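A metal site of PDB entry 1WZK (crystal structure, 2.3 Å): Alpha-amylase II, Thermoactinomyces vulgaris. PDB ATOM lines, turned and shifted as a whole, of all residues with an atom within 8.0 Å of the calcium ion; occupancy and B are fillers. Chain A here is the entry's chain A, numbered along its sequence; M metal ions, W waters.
Water W1 bridges the backbone carbonyl oxygen of Gln 215 (2.5 Å) and the backbone carbonyl oxygen of Asn 148 (3.5 Å).
The calcium ion is bound by the side-chain amide oxygen of Asn 148 (2.2 Å), the side-chain carboxylate of Asp 149 (2.2 Å), water W1 (2.4 Å), the side-chain carboxylate of Asp 171 (2.4 Å), the side-chain amide oxygen of Asn 143 (2.5 Å), the backbone carbonyl oxygen of Asp 145 (2.5 Å) and the backbone carbonyl oxygen of Gly 169 (2.5 Å).
The calcium ion has seven donor atoms within binding distance.
O of Gln 215 sits close to ND2 of Asn 148 (3.4 Å).
OD1 of Asp 171 is in hydrogen-bond range of N of Gly 144.
N of Asp 171 lies within hydrogen-bond range of O of Ala 142, 3.0 Å away.
The side-chain carboxylate (OD1) of Asp 171 is in hydrogen-bond range of the backbone NH (N) of Lys 173, 3.3 Å away.
OD1 of Asp 171 lies within hydrogen-bond range of N of Gly 174 (2.7 Å).
The backbone carbonyl oxygen (O) of Pro 138 sits at hydrogen-bond distance from the backbone NH (N) of Asp 171, 3.4 Å away.
The side-chain carboxylate (OD1) of Asp 145 sits at hydrogen-bond distance from the side-chain hydroxyl (OG) of Ser 147 (2.6 Å).
The backbone NH (N) of Gly 169 is in hydrogen-bond range of the side-chain carboxylate (OE1) of Glu 139 (3.0 Å).
Six residues have an atom within 4 Å of the calcium ion: Asn 143, Asp 145, Asn 148, Asp 149, Gly 169 and Asp 171.
The nearest printed residue that does not touch the calcium ion is Pro 146 (4.2 Å).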
ATOM      1  N   PRO A 138      26.453  20.202  14.069  1.00  0.00           N
ATOM      2  CA  PRO A 138      25.462  19.124  14.024  1.00  0.00           C
ATOM      3  C   PRO A 138      25.304  18.324  12.745  1.00  0.00           C
ATOM      4  O   PRO A 138      25.259  17.101  12.787  1.00  0.00           O
ATOM      5  CB  PRO A 138      24.168  19.818  14.458  1.00  0.00           C
ATOM      6  CG  PRO A 138      24.385  21.235  14.048  1.00  0.00           C
ATOM      7  CD  PRO A 138      25.812  21.488  14.397  1.00  0.00           C
ATOM      8  N   GLU A 139      25.248  18.995  11.596  1.00  0.00           N
ATOM      9  CA  GLU A 139      25.103  18.278  10.327  1.00  0.00           C
ATOM     10  C   GLU A 139      26.209  17.257  10.109  1.00  0.00           C
ATOM     11  O   GLU A 139      26.004  16.261   9.410  1.00  0.00           O
ATOM     12  CB  GLU A 139      25.081  19.265   9.153  1.00  0.00           C
ATOM     13  CG  GLU A 139      24.012  18.996   8.080  1.00  0.00           C
ATOM     14  CD  GLU A 139      24.234  17.687   7.328  1.00  0.00           C
ATOM     15  OE1 GLU A 139      23.365  16.796   7.415  1.00  0.00           O
ATOM     16  OE2 GLU A 139      25.283  17.553   6.658  1.00  0.00           O
ATOM     17  N   ALA A 142      27.539  13.458  14.177  1.00  0.00           N
ATOM     18  CA  ALA A 142      27.097  12.070  14.282  1.00  0.00           C
ATOM     19  C   ALA A 142      25.658  11.910  13.797  1.00  0.00           C
ATOM     20  O   ALA A 142      24.774  12.682  14.181  1.00  0.00           O
ATOM     21  CB  ALA A 142      27.214  11.587  15.726  1.00  0.00           C
ATOM     22  N   ASN A 143      25.417  10.903  12.955  1.00  0.00           N
ATOM     23  CA  ASN A 143      24.076  10.642  12.417  1.00  0.00           C
ATOM     24  C   ASN A 143      23.471   9.474  13.198  1.00  0.00           C
ATOM     25  O   ASN A 143      23.663   8.319  12.829  1.00  0.00           O
ATOM     26  CB  ASN A 143      24.146  10.266  10.930  1.00  0.00           C
ATOM     27  CG  ASN A 143      22.772  10.075  10.287  1.00  0.00           C
ATOM     28  OD1 ASN A 143      21.738  10.263  10.935  1.00  0.00           O
ATOM     29  ND2 ASN A 143      22.767   9.709   9.012  1.00  0.00           N
ATOM     30  N   GLY A 144      22.743   9.786  14.266  1.00  0.00           N
ATOM     31  CA  GLY A 144      22.140   8.744  15.064  1.00  0.00           C
ATOM     32  C   GLY A 144      20.790   8.308  14.531  1.00  0.00           C
ATOM     33  O   GLY A 144      20.311   7.221  14.853  1.00  0.00           O
ATOM     34  N   ASP A 145      20.185   9.165  13.702  1.00  0.00           N
ATOM     35  CA  ASP A 145      18.872   8.889  13.131  1.00  0.00           C
ATOM     36  C   ASP A 145      18.829   9.059  11.623  1.00  0.00           C
ATOM     37  O   ASP A 145      18.626  10.150  11.121  1.00  0.00           O
ATOM     38  CB  ASP A 145      17.832   9.807  13.782  1.00  0.00           C
ATOM     39  CG  ASP A 145      16.417   9.462  13.369  1.00  0.00           C
ATOM     40  OD1 ASP A 145      16.246   8.463  12.642  1.00  0.00           O
ATOM     41  OD2 ASP A 145      15.486  10.197  13.786  1.00  0.00           O
ATOM     42  N   PRO A 146      19.009   7.956  10.880  1.00  0.00           N
ATOM     43  CA  PRO A 146      18.978   8.001   9.412  1.00  0.00           C
ATOM     44  C   PRO A 146      17.617   8.405   8.829  1.00  0.00           C
ATOM     45  O   PRO A 146      17.549   8.911   7.706  1.00  0.00           O
ATOM     46  CB  PRO A 146      19.351   6.573   9.012  1.00  0.00           C
ATOM     47  CG  PRO A 146      20.119   6.058  10.180  1.00  0.00           C
ATOM     48  CD  PRO A 146      19.360   6.608  11.361  1.00  0.00           C
ATOM     49  N   SER A 147      16.539   8.177   9.568  1.00  0.00           N
ATOM     50  CA  SER A 147      15.196   8.492   9.071  1.00  0.00           C
ATOM     51  C   SER A 147      14.899   9.980   8.907  1.00  0.00           C
ATOM     52  O   SER A 147      13.892  10.338   8.306  1.00  0.00           O
ATOM     53  CB  SER A 147      14.134   7.869   9.977  1.00  0.00           C
ATOM     54  OG  SER A 147      14.061   8.544  11.217  1.00  0.00           O
ATOM     55  N   ASN A 148      15.764  10.853   9.445  1.00  0.00           N
ATOM     56  CA  ASN A 148      15.530  12.291   9.311  1.00  0.00           C
ATOM     57  C   ASN A 148      16.513  12.950   8.347  1.00  0.00           C
ATOM     58  O   ASN A 148      16.553  14.177   8.247  1.00  0.00           O
ATOM     59  CB  ASN A 148      15.607  12.995  10.674  1.00  0.00           C
ATOM     60  CG  ASN A 148      16.978  12.917  11.322  1.00  0.00           C
ATOM     61  OD1 ASN A 148      17.992  12.722  10.653  1.00  0.00           O
ATOM     62  ND2 ASN A 148      17.024  13.083  12.643  1.00  0.00           N
ATOM     63  N   ASP A 149      17.306  12.148   7.642  1.00  0.00           N
ATOM     64  CA  ASP A 149      18.283  12.695   6.709  1.00  0.00           C
ATOM     65  C   ASP A 149      17.659  13.472   5.562  1.00  0.00           C
ATOM     66  O   ASP A 149      16.610  13.111   5.034  1.00  0.00           O
ATOM     67  CB  ASP A 149      19.158  11.563   6.149  1.00  0.00           C
ATOM     68  CG  ASP A 149      19.987  10.885   7.216  1.00  0.00           C
ATOM     69  OD1 ASP A 149      20.748   9.966   6.885  1.00  0.00           O
ATOM     70  OD2 ASP A 149      19.883  11.295   8.388  1.00  0.00           O
ATOM     71  N   PRO A 150      18.298  14.594   5.175  1.00  0.00           N
ATOM     72  CA  PRO A 150      17.770  15.407   4.076  1.00  0.00           C
ATOM     73  C   PRO A 150      17.837  14.590   2.786  1.00  0.00           C
ATOM     74  O   PRO A 150      18.636  13.663   2.672  1.00  0.00           O
ATOM     75  CB  PRO A 150      18.720  16.597   4.046  1.00  0.00           C
ATOM     76  CG  PRO A 150      19.175  16.710   5.460  1.00  0.00           C
ATOM     77  CD  PRO A 150      19.419  15.276   5.829  1.00  0.00           C
ATOM     78  N   THR A 153      21.220  12.646   0.932  1.00  0.00           N
ATOM     79  CA  THR A 153      22.305  12.580   1.899  1.00  0.00           C
ATOM     80  C   THR A 153      23.408  11.680   1.347  1.00  0.00           C
ATOM     81  O   THR A 153      23.126  10.558   0.922  1.00  0.00           O
ATOM     82  CB  THR A 153      21.824  11.971   3.221  1.00  0.00           C
ATOM     83  OG1 THR A 153      20.880  12.857   3.852  1.00  0.00           O
ATOM     84  CG2 THR A 153      22.988  11.714   4.162  1.00  0.00           C
ATOM     85  N   TRP A 156      28.702   8.591   4.614  1.00  0.00           N
ATOM     86  CA  TRP A 156      29.510   9.074   5.724  1.00  0.00           C
ATOM     87  C   TRP A 156      30.832   8.309   5.746  1.00  0.00           C
ATOM     88  O   TRP A 156      30.916   7.211   6.302  1.00  0.00           O
ATOM     89  CB  TRP A 156      28.744   8.870   7.041  1.00  0.00           C
ATOM     90  CG  TRP A 156      29.339   9.568   8.234  1.00  0.00           C
ATOM     91  CD1 TRP A 156      30.538   9.296   8.828  1.00  0.00           C
ATOM     92  CD2 TRP A 156      28.758  10.654   8.974  1.00  0.00           C
ATOM     93  NE1 TRP A 156      30.740  10.141   9.893  1.00  0.00           N
ATOM     94  CE2 TRP A 156      29.659  10.980  10.011  1.00  0.00           C
ATOM     95  CE3 TRP A 156      27.562  11.366   8.857  1.00  0.00           C
ATOM     96  CZ2 TRP A 156      29.407  11.999  10.929  1.00  0.00           C
ATOM     97  CZ3 TRP A 156      27.304  12.398   9.773  1.00  0.00           C
ATOM     98  CH2 TRP A 156      28.231  12.694  10.794  1.00  0.00           C
ATOM     99  N   TYR A 168      25.201  14.919   5.124  1.00  0.00           N
ATOM    100  CA  TYR A 168      25.670  13.655   5.674  1.00  0.00           C
ATOM    101  C   TYR A 168      24.737  13.080   6.735  1.00  0.00           C
ATOM    102  O   TYR A 168      24.939  11.968   7.211  1.00  0.00           O
ATOM    103  CB  TYR A 168      27.067  13.836   6.227  1.00  0.00           C
ATOM    104  CG  TYR A 168      28.066  14.114   5.127  1.00  0.00           C
ATOM    105  CD1 TYR A 168      28.516  13.072   4.305  1.00  0.00           C
ATOM    106  CD2 TYR A 168      28.507  15.404   4.873  1.00  0.00           C
ATOM    107  CE1 TYR A 168      29.382  13.325   3.241  1.00  0.00           C
ATOM    108  CE2 TYR A 168      29.370  15.664   3.815  1.00  0.00           C
ATOM    109  CZ  TYR A 168      29.808  14.627   3.014  1.00  0.00           C
ATOM    110  OH  TYR A 168      30.673  14.884   1.978  1.00  0.00           O
ATOM    111  N   GLY A 169      23.721  13.842   7.103  1.00  0.00           N
ATOM    112  CA  GLY A 169      22.754  13.365   8.076  1.00  0.00           C
ATOM    113  C   GLY A 169      23.061  13.568   9.543  1.00  0.00           C
ATOM    114  O   GLY A 169      22.441  12.942  10.399  1.00  0.00           O
ATOM    115  N   GLY A 170      24.009  14.455   9.845  1.00  0.00           N
ATOM    116  CA  GLY A 170      24.334  14.720  11.231  1.00  0.00           C
ATOM    117  C   GLY A 170      23.097  15.211  11.963  1.00  0.00           C
ATOM    118  O   GLY A 170      22.317  15.994  11.405  1.00  0.00           O
ATOM    119  N   ASP A 171      22.891  14.738  13.202  1.00  0.00           N
ATOM    120  CA  ASP A 171      21.716  15.116  13.988  1.00  0.00           C
ATOM    121  C   ASP A 171      21.890  15.022  15.518  1.00  0.00           C
ATOM    122  O   ASP A 171      22.926  14.537  16.003  1.00  0.00           O
ATOM    123  CB  ASP A 171      20.535  14.229  13.565  1.00  0.00           C
ATOM    124  CG  ASP A 171      20.822  12.760  13.733  1.00  0.00           C
ATOM    125  OD1 ASP A 171      21.476  12.399  14.731  1.00  0.00           O
ATOM    126  OD2 ASP A 171      20.406  11.972  12.874  1.00  0.00           O
ATOM    127  N   LEU A 172      20.871  15.446  16.259  1.00  0.00           N
ATOM    128  CA  LEU A 172      20.909  15.428  17.716  1.00  0.00           C
ATOM    129  C   LEU A 172      20.968  14.023  18.325  1.00  0.00           C
ATOM    130  O   LEU A 172      21.625  13.809  19.365  1.00  0.00           O
ATOM    131  CB  LEU A 172      19.705  16.180  18.301  1.00  0.00           C
ATOM    132  CG  LEU A 172      19.625  17.665  17.901  1.00  0.00           C
ATOM    133  CD1 LEU A 172      18.441  18.325  18.594  1.00  0.00           C
ATOM    134  CD2 LEU A 172      20.943  18.382  18.312  1.00  0.00           C
ATOM    135  N   LYS A 173      20.306  13.060  17.700  1.00  0.00           N
ATOM    136  CA  LYS A 173      20.353  11.691  18.224  1.00  0.00           C
ATOM    137  C   LYS A 173      21.810  11.219  18.191  1.00  0.00           C
ATOM    138  O   LYS A 173      22.274  10.527  19.105  1.00  0.00           O
ATOM    139  CB  LYS A 173      19.484  10.735  17.399  1.00  0.00           C
ATOM    140  CG  LYS A 173      19.446   9.296  17.974  1.00  0.00           C
ATOM    141  CD  LYS A 173      18.882   9.254  19.401  1.00  0.00           C
ATOM    142  CE  LYS A 173      19.318   8.008  20.163  1.00  0.00           C
ATOM    143  NZ  LYS A 173      19.066   6.737  19.432  1.00  0.00           N
ATOM    144  N   GLY A 174      22.514  11.605  17.138  1.00  0.00           N
ATOM    145  CA  GLY A 174      23.916  11.227  17.024  1.00  0.00           C
ATOM    146  C   GLY A 174      24.712  11.801  18.185  1.00  0.00           C
ATOM    147  O   GLY A 174      25.525  11.107  18.773  1.00  0.00           O
ATOM    148  N   PRO A 214      13.672  19.729  11.614  1.00  0.00           N
ATOM    149  CA  PRO A 214      13.331  18.318  11.453  1.00  0.00           C
ATOM    150  C   PRO A 214      14.488  17.399  11.092  1.00  0.00           C
ATOM    151  O   PRO A 214      14.519  16.241  11.520  1.00  0.00           O
ATOM    152  CB  PRO A 214      12.263  18.339  10.351  1.00  0.00           C
ATOM    153  CG  PRO A 214      11.575  19.644  10.611  1.00  0.00           C
ATOM    154  CD  PRO A 214      12.733  20.579  10.862  1.00  0.00           C
ATOM    155  N   GLN A 215      15.443  17.896  10.323  1.00  0.00           N
ATOM    156  CA  GLN A 215      16.576  17.043   9.951  1.00  0.00           C
ATOM    157  C   GLN A 215      17.509  16.816  11.138  1.00  0.00           C
ATOM    158  O   GLN A 215      18.306  15.883  11.133  1.00  0.00           O
ATOM    159  CB  GLN A 215      17.364  17.666   8.779  1.00  0.00           C
ATOM    160  CG  GLN A 215      18.378  18.716   9.209  1.00  0.00           C
ATOM    161  CD  GLN A 215      19.031  19.419   8.027  1.00  0.00           C
ATOM    162  OE1 GLN A 215      18.393  20.223   7.327  1.00  0.00           O
ATOM    163  NE2 GLN A 215      20.304  19.123   7.804  1.00  0.00           N
ATOM    164  N   PHE A 216      17.424  17.683  12.156  1.00  0.00           N
ATOM    165  CA  PHE A 216      18.292  17.533  13.329  1.00  0.00           C
ATOM    166  C   PHE A 216      17.608  16.800  14.478  1.00  0.00           C
ATOM    167  O   PHE A 216      18.241  16.030  15.202  1.00  0.00           O
ATOM    168  CB  PHE A 216      18.788  18.898  13.823  1.00  0.00           C
ATOM    169  CG  PHE A 216      19.794  19.563  12.916  1.00  0.00           C
ATOM    170  CD1 PHE A 216      20.819  18.825  12.323  1.00  0.00           C
ATOM    171  CD2 PHE A 216      19.746  20.943  12.712  1.00  0.00           C
ATOM    172  CE1 PHE A 216      21.791  19.459  11.534  1.00  0.00           C
ATOM    173  CE2 PHE A 216      20.714  21.584  11.928  1.00  0.00           C
ATOM    174  CZ  PHE A 216      21.746  20.834  11.337  1.00  0.00           C
ATOM    175  N   GLY A 217      16.314  17.025  14.640  1.00  0.00           N
ATOM    176  CA  GLY A 217      15.573  16.367  15.698  1.00  0.00           C
ATOM    177  C   GLY A 217      14.260  17.082  15.978  1.00  0.00           C
ATOM    178  O   GLY A 217      13.656  17.676  15.082  1.00  0.00           O
HETATM  179 CA    CA M   1      20.093  12.032  10.479  1.00  0.00          CA
HETATM  180  O   HOH W   1      19.713  14.296   9.729  1.00  0.00           O
